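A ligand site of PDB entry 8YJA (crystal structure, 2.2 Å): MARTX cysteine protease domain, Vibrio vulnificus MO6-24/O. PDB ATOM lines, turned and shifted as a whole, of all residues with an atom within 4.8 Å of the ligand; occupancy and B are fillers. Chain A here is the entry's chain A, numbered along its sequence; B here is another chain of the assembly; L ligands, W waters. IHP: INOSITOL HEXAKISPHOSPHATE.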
ATOM      1  N   GLU A  29      18.691  19.531 -29.395  1.00  0.00           N
ATOM      2  CA  GLU A  29      20.010  18.898 -29.454  1.00  0.00           C
ATOM      3  C   GLU A  29      20.137  17.774 -28.416  1.00  0.00           C
ATOM      4  O   GLU A  29      19.283  16.895 -28.302  1.00  0.00           O
ATOM      5  CB  GLU A  29      21.119  19.924 -29.195  1.00  0.00           C
ATOM      6  CG  GLU A  29      20.943  21.274 -29.875  1.00  0.00           C
ATOM      7  CD  GLU A  29      22.002  22.277 -29.434  1.00  0.00           C
ATOM      8  OE1 GLU A  29      22.969  21.864 -28.746  1.00  0.00           O
ATOM      9  OE2 GLU A  29      21.882  23.475 -29.762  1.00  0.00           O
ATOM     10  N   SER A  30      21.226  17.854 -27.659  1.00  0.00           N
ATOM     11  CA  SER A  30      21.449  17.032 -26.472  1.00  0.00           C
ATOM     12  C   SER A  30      21.794  17.970 -25.320  1.00  0.00           C
ATOM     13  O   SER A  30      22.191  19.120 -25.514  1.00  0.00           O
ATOM     14  CB  SER A  30      22.579  16.009 -26.693  1.00  0.00           C
ATOM     15  OG  SER A  30      22.495  14.924 -25.780  1.00  0.00           O
ATOM     16  N   ARG A  31      21.607  17.468 -24.089  1.00  0.00           N
ATOM     17  CA  ARG A  31      22.054  18.201 -22.901  1.00  0.00           C
ATOM     18  C   ARG A  31      23.519  17.935 -22.596  1.00  0.00           C
ATOM     19  O   ARG A  31      24.064  18.545 -21.664  1.00  0.00           O
ATOM     20  CB  ARG A  31      21.193  17.836 -21.688  1.00  0.00           C
ATOM     21  CG  ARG A  31      21.263  16.377 -21.239  1.00  0.00           C
ATOM     22  CD  ARG A  31      20.057  16.049 -20.364  1.00  0.00           C
ATOM     23  NE  ARG A  31      20.159  14.764 -19.683  1.00  0.00           N
ATOM     24  CZ  ARG A  31      20.923  14.523 -18.619  1.00  0.00           C
ATOM     25  NH1 ARG A  31      21.697  15.477 -18.103  1.00  0.00           N
ATOM     26  NH2 ARG A  31      20.910  13.317 -18.066  1.00  0.00           N
ATOM     27  N   PHE A  32      24.157  17.049 -23.350  1.00  0.00           N
ATOM     28  CA  PHE A  32      25.582  16.792 -23.271  1.00  0.00           C
ATOM     29  C   PHE A  32      26.298  17.513 -24.396  1.00  0.00           C
ATOM     30  O   PHE A  32      25.827  17.515 -25.535  1.00  0.00           O
ATOM     31  CB  PHE A  32      25.852  15.282 -23.342  1.00  0.00           C
ATOM     32  CG  PHE A  32      25.049  14.488 -22.356  1.00  0.00           C
ATOM     33  CD1 PHE A  32      25.458  14.389 -21.027  1.00  0.00           C
ATOM     34  CD2 PHE A  32      23.885  13.852 -22.744  1.00  0.00           C
ATOM     35  CE1 PHE A  32      24.714  13.664 -20.112  1.00  0.00           C
ATOM     36  CE2 PHE A  32      23.144  13.115 -21.836  1.00  0.00           C
ATOM     37  CZ  PHE A  32      23.557  13.029 -20.512  1.00  0.00           C
ATOM     38  N   LYS A  56      24.285  10.358 -34.550  1.00  0.00           N
ATOM     39  CA  LYS A  56      23.274  11.274 -34.061  1.00  0.00           C
ATOM     40  C   LYS A  56      23.869  12.604 -33.654  1.00  0.00           C
ATOM     41  O   LYS A  56      23.156  13.611 -33.661  1.00  0.00           O
ATOM     42  CB  LYS A  56      22.490  10.670 -32.890  1.00  0.00           C
ATOM     43  CG  LYS A  56      21.932   9.299 -33.180  1.00  0.00           C
ATOM     44  CD  LYS A  56      20.701   9.052 -32.342  1.00  0.00           C
ATOM     45  CE  LYS A  56      19.479   8.855 -33.224  1.00  0.00           C
ATOM     46  NZ  LYS A  56      19.506   7.541 -33.923  1.00  0.00           N
ATOM     47  N   HIS A  57      25.137  12.631 -33.260  1.00  0.00           N
ATOM     48  CA  HIS A  57      25.832  13.872 -32.904  1.00  0.00           C
ATOM     49  C   HIS A  57      27.217  13.846 -33.547  1.00  0.00           C
ATOM     50  O   HIS A  57      28.242  13.803 -32.861  1.00  0.00           O
ATOM     51  CB  HIS A  57      25.924  14.031 -31.382  1.00  0.00           C
ATOM     52  CG  HIS A  57      24.579  14.036 -30.717  1.00  0.00           C
ATOM     53  ND1 HIS A  57      23.820  12.892 -30.564  1.00  0.00           N
ATOM     54  CD2 HIS A  57      23.852  15.046 -30.189  1.00  0.00           C
ATOM     55  CE1 HIS A  57      22.690  13.192 -29.967  1.00  0.00           C
ATOM     56  NE2 HIS A  57      22.677  14.491 -29.723  1.00  0.00           N
ATOM     57  N   ARG A  87      29.110  12.663 -21.974  1.00  0.00           N
ATOM     58  CA  ARG A  87      28.490  11.357 -21.786  1.00  0.00           C
ATOM     59  C   ARG A  87      29.428  10.287 -22.311  1.00  0.00           C
ATOM     60  O   ARG A  87      30.193  10.513 -23.256  1.00  0.00           O
ATOM     61  CB  ARG A  87      27.140  11.283 -22.527  1.00  0.00           C
ATOM     62  CG  ARG A  87      26.522   9.875 -22.584  1.00  0.00           C
ATOM     63  CD  ARG A  87      25.075   9.893 -23.101  1.00  0.00           C
ATOM     64  NE  ARG A  87      24.967  10.491 -24.432  1.00  0.00           N
ATOM     65  CZ  ARG A  87      23.816  10.678 -25.072  1.00  0.00           C
ATOM     66  NH1 ARG A  87      22.659  10.331 -24.527  1.00  0.00           N
ATOM     67  NH2 ARG A  87      23.822  11.243 -26.282  1.00  0.00           N
ATOM     68  N   GLN A  89      28.962   6.296 -23.757  1.00  0.00           N
ATOM     69  CA  GLN A  89      28.096   5.190 -24.142  1.00  0.00           C
ATOM     70  C   GLN A  89      28.975   3.978 -24.394  1.00  0.00           C
ATOM     71  O   GLN A  89      29.841   4.015 -25.286  1.00  0.00           O
ATOM     72  CB  GLN A  89      27.274   5.533 -25.398  1.00  0.00           C
ATOM     73  CG  GLN A  89      26.500   6.853 -25.296  1.00  0.00           C
ATOM     74  CD  GLN A  89      25.144   6.792 -25.975  1.00  0.00           C
ATOM     75  OE1 GLN A  89      24.370   5.851 -25.777  1.00  0.00           O
ATOM     76  NE2 GLN A  89      24.832   7.804 -26.771  1.00  0.00           N
ATOM     77  N   HIS A 136      27.521  11.033 -17.213  1.00  0.00           N
ATOM     78  CA  HIS A 136      26.501  10.033 -17.511  1.00  0.00           C
ATOM     79  C   HIS A 136      27.126   8.913 -18.325  1.00  0.00           C
ATOM     80  O   HIS A 136      27.953   9.153 -19.211  1.00  0.00           O
ATOM     81  CB  HIS A 136      25.333  10.670 -18.266  1.00  0.00           C
ATOM     82  CG  HIS A 136      24.176   9.735 -18.486  1.00  0.00           C
ATOM     83  ND1 HIS A 136      23.008   9.826 -17.768  1.00  0.00           N
ATOM     84  CD2 HIS A 136      24.035   8.689 -19.330  1.00  0.00           C
ATOM     85  CE1 HIS A 136      22.178   8.865 -18.162  1.00  0.00           C
ATOM     86  NE2 HIS A 136      22.776   8.171 -19.113  1.00  0.00           N
ATOM     87  N   SER A 138      25.838   5.502 -20.432  1.00  0.00           N
ATOM     88  CA  SER A 138      24.784   4.651 -20.965  1.00  0.00           C
ATOM     89  C   SER A 138      25.411   3.358 -21.441  1.00  0.00           C
ATOM     90  O   SER A 138      26.352   3.379 -22.243  1.00  0.00           O
ATOM     91  CB  SER A 138      24.044   5.309 -22.129  1.00  0.00           C
ATOM     92  OG  SER A 138      23.461   6.524 -21.719  1.00  0.00           O
ATOM     93  N   SER A 171      22.458   4.461 -17.124  1.00  0.00           N
ATOM     94  CA  SER A 171      21.265   3.806 -17.651  1.00  0.00           C
ATOM     95  C   SER A 171      21.681   2.640 -18.526  1.00  0.00           C
ATOM     96  O   SER A 171      22.790   2.609 -19.081  1.00  0.00           O
ATOM     97  CB  SER A 171      20.384   4.784 -18.442  1.00  0.00           C
ATOM     98  OG  SER A 171      21.048   5.183 -19.618  1.00  0.00           O
ATOM     99  N   ARG A 173      20.178  -0.053 -21.574  1.00  0.00           N
ATOM    100  CA  ARG A 173      19.120  -0.325 -22.536  1.00  0.00           C
ATOM    101  C   ARG A 173      19.629  -1.266 -23.615  1.00  0.00           C
ATOM    102  O   ARG A 173      20.806  -1.629 -23.652  1.00  0.00           O
ATOM    103  CB  ARG A 173      18.614   0.961 -23.192  1.00  0.00           C
ATOM    104  CG  ARG A 173      19.700   1.741 -23.891  1.00  0.00           C
ATOM    105  CD  ARG A 173      19.114   2.872 -24.700  1.00  0.00           C
ATOM    106  NE  ARG A 173      20.152   3.823 -25.073  1.00  0.00           N
ATOM    107  CZ  ARG A 173      20.591   4.004 -26.307  1.00  0.00           C
ATOM    108  NH1 ARG A 173      20.072   3.315 -27.324  1.00  0.00           N
ATOM    109  NH2 ARG A 173      21.553   4.886 -26.530  1.00  0.00           N
ATOM    110  N   GLU B  29      12.597  12.834 -30.623  1.00  0.00           N
ATOM    111  CA  GLU B  29      12.079  11.473 -30.663  1.00  0.00           C
ATOM    112  C   GLU B  29      12.703  10.608 -29.561  1.00  0.00           C
ATOM    113  O   GLU B  29      13.868  10.199 -29.654  1.00  0.00           O
ATOM    114  CB  GLU B  29      12.318  10.853 -32.041  1.00  0.00           C
ATOM    115  CG  GLU B  29      11.943   9.379 -32.174  1.00  0.00           C
ATOM    116  CD  GLU B  29      10.485   9.057 -31.796  1.00  0.00           C
ATOM    117  OE1 GLU B  29       9.676   9.993 -31.583  1.00  0.00           O
ATOM    118  OE2 GLU B  29      10.160   7.856 -31.717  1.00  0.00           O
ATOM    119  N   ARG B  31      13.219   7.532 -26.639  1.00  0.00           N
ATOM    120  CA  ARG B  31      13.226   6.068 -26.590  1.00  0.00           C
ATOM    121  C   ARG B  31      12.238   5.508 -25.582  1.00  0.00           C
ATOM    122  O   ARG B  31      12.150   4.285 -25.443  1.00  0.00           O
ATOM    123  CB  ARG B  31      14.638   5.551 -26.288  1.00  0.00           C
ATOM    124  CG  ARG B  31      15.067   5.761 -24.852  1.00  0.00           C
ATOM    125  CD  ARG B  31      16.464   5.211 -24.599  1.00  0.00           C
ATOM    126  NE  ARG B  31      16.914   5.403 -23.225  1.00  0.00           N
ATOM    127  CZ  ARG B  31      16.670   4.571 -22.226  1.00  0.00           C
ATOM    128  NH1 ARG B  31      15.981   3.444 -22.399  1.00  0.00           N
ATOM    129  NH2 ARG B  31      17.147   4.863 -21.006  1.00  0.00           N
ATOM    130  N   PHE B  32      11.504   6.359 -24.850  1.00  0.00           N
ATOM    131  CA  PHE B  32      10.377   5.928 -24.038  1.00  0.00           C
ATOM    132  C   PHE B  32       9.089   6.154 -24.820  1.00  0.00           C
ATOM    133  O   PHE B  32       9.006   7.073 -25.635  1.00  0.00           O
ATOM    134  CB  PHE B  32      10.343   6.681 -22.698  1.00  0.00           C
ATOM    135  CG  PHE B  32      11.606   6.507 -21.888  1.00  0.00           C
ATOM    136  CD1 PHE B  32      11.813   5.356 -21.138  1.00  0.00           C
ATOM    137  CD2 PHE B  32      12.600   7.468 -21.930  1.00  0.00           C
ATOM    138  CE1 PHE B  32      12.986   5.176 -20.428  1.00  0.00           C
ATOM    139  CE2 PHE B  32      13.763   7.300 -21.201  1.00  0.00           C
ATOM    140  CZ  PHE B  32      13.968   6.145 -20.460  1.00  0.00           C
ATOM    141  N   ARG B  87       8.986   6.228 -18.554  1.00  0.00           N
ATOM    142  CA  ARG B  87       9.826   6.851 -17.553  1.00  0.00           C
ATOM    143  C   ARG B  87       8.975   7.751 -16.676  1.00  0.00           C
ATOM    144  O   ARG B  87       7.868   8.143 -17.045  1.00  0.00           O
ATOM    145  CB  ARG B  87      10.963   7.657 -18.174  1.00  0.00           C
ATOM    146  CG  ARG B  87      10.565   9.012 -18.703  1.00  0.00           C
ATOM    147  CD  ARG B  87      11.779   9.833 -19.127  1.00  0.00           C
ATOM    148  NE  ARG B  87      11.385  10.764 -20.180  1.00  0.00           N
ATOM    149  CZ  ARG B  87      12.240  11.454 -20.929  1.00  0.00           C
ATOM    150  NH1 ARG B  87      13.549  11.344 -20.774  1.00  0.00           N
ATOM    151  NH2 ARG B  87      11.758  12.269 -21.856  1.00  0.00           N
ATOM    152  N   GLN B  89       9.456  11.480 -14.609  1.00  0.00           N
ATOM    153  CA  GLN B  89      10.244  12.642 -14.251  1.00  0.00           C
ATOM    154  C   GLN B  89       9.641  13.255 -12.996  1.00  0.00           C
ATOM    155  O   GLN B  89       8.441  13.576 -12.982  1.00  0.00           O
ATOM    156  CB  GLN B  89      10.315  13.645 -15.392  1.00  0.00           C
ATOM    157  CG  GLN B  89      10.584  12.978 -16.746  1.00  0.00           C
ATOM    158  CD  GLN B  89      11.452  13.834 -17.637  1.00  0.00           C
ATOM    159  OE1 GLN B  89      12.533  14.240 -17.243  1.00  0.00           O
ATOM    160  NE2 GLN B  89      10.968  14.123 -18.851  1.00  0.00           N
ATOM    161  N   HIS B 136      12.702   3.975 -15.957  1.00  0.00           N
ATOM    162  CA  HIS B 136      13.659   5.037 -15.693  1.00  0.00           C
ATOM    163  C   HIS B 136      12.951   6.118 -14.902  1.00  0.00           C
ATOM    164  O   HIS B 136      11.769   6.405 -15.128  1.00  0.00           O
ATOM    165  CB  HIS B 136      14.230   5.616 -17.008  1.00  0.00           C
ATOM    166  CG  HIS B 136      15.254   6.686 -16.803  1.00  0.00           C
ATOM    167  ND1 HIS B 136      16.610   6.463 -16.973  1.00  0.00           N
ATOM    168  CD2 HIS B 136      15.135   7.979 -16.416  1.00  0.00           C
ATOM    169  CE1 HIS B 136      17.277   7.579 -16.716  1.00  0.00           C
ATOM    170  NE2 HIS B 136      16.407   8.516 -16.382  1.00  0.00           N
ATOM    171  N   SER B 138      13.663  10.131 -13.763  1.00  0.00           N
ATOM    172  CA  SER B 138      14.479  11.332 -13.818  1.00  0.00           C
ATOM    173  C   SER B 138      14.121  12.239 -12.648  1.00  0.00           C
ATOM    174  O   SER B 138      12.951  12.407 -12.319  1.00  0.00           O
ATOM    175  CB  SER B 138      14.287  12.073 -15.143  1.00  0.00           C
ATOM    176  OG  SER B 138      14.774  11.256 -16.199  1.00  0.00           O
ATOM    177  N   SER B 171      18.381   9.168 -13.263  1.00  0.00           N
ATOM    178  CA  SER B 171      19.262  10.262 -13.617  1.00  0.00           C
ATOM    179  C   SER B 171      18.852  11.502 -12.825  1.00  0.00           C
ATOM    180  O   SER B 171      17.713  11.613 -12.383  1.00  0.00           O
ATOM    181  CB  SER B 171      19.240  10.543 -15.115  1.00  0.00           C
ATOM    182  OG  SER B 171      17.914  10.673 -15.547  1.00  0.00           O
ATOM    183  N   ARG B 173      19.362  15.837 -12.903  1.00  0.00           N
ATOM    184  CA  ARG B 173      19.826  16.973 -13.692  1.00  0.00           C
ATOM    185  C   ARG B 173      19.185  18.260 -13.167  1.00  0.00           C
ATOM    186  O   ARG B 173      18.308  18.236 -12.289  1.00  0.00           O
ATOM    187  CB  ARG B 173      19.506  16.784 -15.179  1.00  0.00           C
ATOM    188  CG  ARG B 173      18.005  16.787 -15.517  1.00  0.00           C
ATOM    189  CD  ARG B 173      17.755  16.980 -17.024  1.00  0.00           C
ATOM    190  NE  ARG B 173      16.466  16.464 -17.455  1.00  0.00           N
ATOM    191  CZ  ARG B 173      15.497  17.182 -18.008  1.00  0.00           C
ATOM    192  NH1 ARG B 173      15.624  18.498 -18.179  1.00  0.00           N
ATOM    193  NH2 ARG B 173      14.390  16.582 -18.420  1.00  0.00           N
HETATM  194  C1  IHP L   1      18.362  10.300 -24.542  1.00  0.00           C
HETATM  195  C2  IHP L   1      17.970  11.779 -24.434  1.00  0.00           C
HETATM  196  C3  IHP L   1      17.167  12.088 -23.175  1.00  0.00           C
HETATM  197  C4  IHP L   1      17.780  11.538 -21.886  1.00  0.00           C
HETATM  198  C5  IHP L   1      18.248  10.079 -21.984  1.00  0.00           C
HETATM  199  C6  IHP L   1      18.971   9.703 -23.289  1.00  0.00           C
HETATM  200  O11 IHP L   1      19.377  10.203 -25.532  1.00  0.00           O
HETATM  201  P1  IHP L   1      19.009   9.220 -26.802  1.00  0.00           P
HETATM  202  O21 IHP L   1      19.962   9.538 -27.940  1.00  0.00           O
HETATM  203  O31 IHP L   1      17.579   9.457 -27.234  1.00  0.00           O
HETATM  204  O41 IHP L   1      19.133   7.786 -26.363  1.00  0.00           O
HETATM  205  O12 IHP L   1      19.157  12.532 -24.379  1.00  0.00           O
HETATM  206  P2  IHP L   1      19.425  13.733 -25.438  1.00  0.00           P
HETATM  207  O22 IHP L   1      20.669  13.404 -26.231  1.00  0.00           O
HETATM  208  O32 IHP L   1      18.234  13.876 -26.370  1.00  0.00           O
HETATM  209  O42 IHP L   1      19.642  14.994 -24.637  1.00  0.00           O
HETATM  210  O13 IHP L   1      17.088  13.515 -23.055  1.00  0.00           O
HETATM  211  P3  IHP L   1      15.598  14.081 -22.533  1.00  0.00           P
HETATM  212  O23 IHP L   1      15.753  14.707 -21.170  1.00  0.00           O
HETATM  213  O33 IHP L   1      14.682  12.873 -22.477  1.00  0.00           O
HETATM  214  O43 IHP L   1      15.027  15.091 -23.506  1.00  0.00           O
HETATM  215  O14 IHP L   1      16.795  11.566 -20.865  1.00  0.00           O
HETATM  216  P4  IHP L   1      17.178  12.175 -19.334  1.00  0.00           P
HETATM  217  O24 IHP L   1      17.298  13.684 -19.425  1.00  0.00           O
HETATM  218  O34 IHP L   1      16.033  11.795 -18.385  1.00  0.00           O
HETATM  219  O44 IHP L   1      18.501  11.649 -18.814  1.00  0.00           O
HETATM  220  O15 IHP L   1      19.172   9.823 -20.945  1.00  0.00           O
HETATM  221  P5  IHP L   1      18.838   8.609 -19.891  1.00  0.00           P
HETATM  222  O25 IHP L   1      17.559   7.908 -20.296  1.00  0.00           O
HETATM  223  O35 IHP L   1      19.966   7.603 -19.878  1.00  0.00           O
HETATM  224  O45 IHP L   1      18.795   9.184 -18.502  1.00  0.00           O
HETATM  225  O16 IHP L   1      18.845   8.311 -23.394  1.00  0.00           O
HETATM  226  P6  IHP L   1      20.178   7.363 -23.063  1.00  0.00           P
HETATM  227  O26 IHP L   1      19.833   6.327 -22.019  1.00  0.00           O
HETATM  228  O36 IHP L   1      20.562   6.649 -24.345  1.00  0.00           O
HETATM  229  O46 IHP L   1      21.321   8.242 -22.601  1.00  0.00           O
HETATM  230  O   HOH W   1      12.795  15.762 -21.234  1.00  0.00           O
HETATM  231  O   HOH W   2      20.334   7.341 -16.005  1.00  0.00           O
HETATM  232  O   HOH W   3      13.144  13.577 -24.330  1.00  0.00           O
HETATM  233  O   HOH W   4      22.041   8.023 -28.224  1.00  0.00           O
HETATM  234  O   HOH W   5      13.928  17.337 -25.068  1.00  0.00           O
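Water W3 bridges O33 of the ligand and NH2 of Arg 87 of chain B. Water W4 lies within hydrogen-bond range of O21 of the ligand (2.6 Å) and NE2 of Gln 89 of chain A (3.2 Å). Water W1 lies within hydrogen-bond range of an oxygen (O23) of the ligand and the guanidinium group (NH2) of Arg 173 of chain B.
Merely in contact with the ligand: Glu 29 of chain A (3.7 Å) and Phe 32 of chain B (3.9 Å). Hydrophobic or aromatic side chains within 4 Å of the ligand: His 136 of chain A, Phe 32 of chain B and His 136 of chain B. Of the 21 residues printed, 15 come within 4 Å of the ligand.
O22 of the ligand sits at hydrogen-bond distance from OG of Ser 30, 2.4 Å away. NH1 of Arg 87 of chain B lies within salt-bridge range of O33 of the ligand. OG of Ser 138 of chain B sits at hydrogen-bond distance from O34 of the ligand (2.6 Å). The side-chain hydroxyl (OG) of Ser 171 of chain A lies within hydrogen-bond range of an oxygen (O35) of the ligand, at 2.7 Å. A ring nitrogen (NE2) of His 136 of chain B lies close to an oxygen (O45) of the ligand (3.3 Å). The side-chain hydroxyl (OG) of Ser 138 of chain A lies within hydrogen-bond range of an oxygen (O46) of the ligand, 2.9 Å away. The guanidinium group (NE) of Arg 173 of chain A is in salt-bridge range of an oxygen (O36) of the ligand (2.9 Å). An oxygen (O35) of the ligand lies within hydrogen-bond range of a ring nitrogen (NE2) of His 136 of chain A, at 3.0 Å. The backbone NH (N) of Arg 31 of chain A lies within hydrogen-bond range of an oxygen (O42) of the ligand (3.2 Å). An oxygen (O44) of the ligand lies within salt-bridge range of the guanidinium group (NH2) of Arg 31 of chain A. An oxygen (O46) of the ligand is in salt-bridge range of the guanidinium group (NH1) of Arg 87 of chain A (3.1 Å). NH2 of Arg 31 of chain B lies within salt-bridge range of O25 of the ligand, 3.2 Å away. The side-chain hydroxyl (OG) of Ser 171 of chain B lies within hydrogen-bond range of an oxygen (O45) of the ligand, 3.4 Å away. An oxygen (O24) of the ligand is in salt-bridge range of the guanidinium group (NE) of Arg 173 of chain B (3.5 Å).
The side-chain hydroxyl (OG) of Ser 138 of chain B is in hydrogen-bond range of a ring nitrogen (NE2) of His 136 of chain B, at 3.2 Å. The side-chain hydroxyl of Ser 138 of chain B sits at hydrogen-bond distance from the side-chain hydroxyl of Ser 171 of chain B. The side-chain hydroxyl (OG) of Ser 138 of chain A sits at hydrogen-bond distance from the side-chain hydroxyl (OG) of Ser 171 of chain A. OG of Ser 171 of chain A sits at hydrogen-bond distance from NE2 of His 136 of chain A. OG of Ser 171 of chain B lies within hydrogen-bond range of NE2 of His 136 of chain B, 2.8 Å away. OG of Ser 138 of chain A is in hydrogen-bond range of NE2 of His 136 of chain A, 3.2 Å away. The guanidinium group (NH2) of Arg 173 of chain A sits at hydrogen-bond distance from the side-chain amide oxygen (OE1) of Gln 89 of chain A (3.1 Å).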
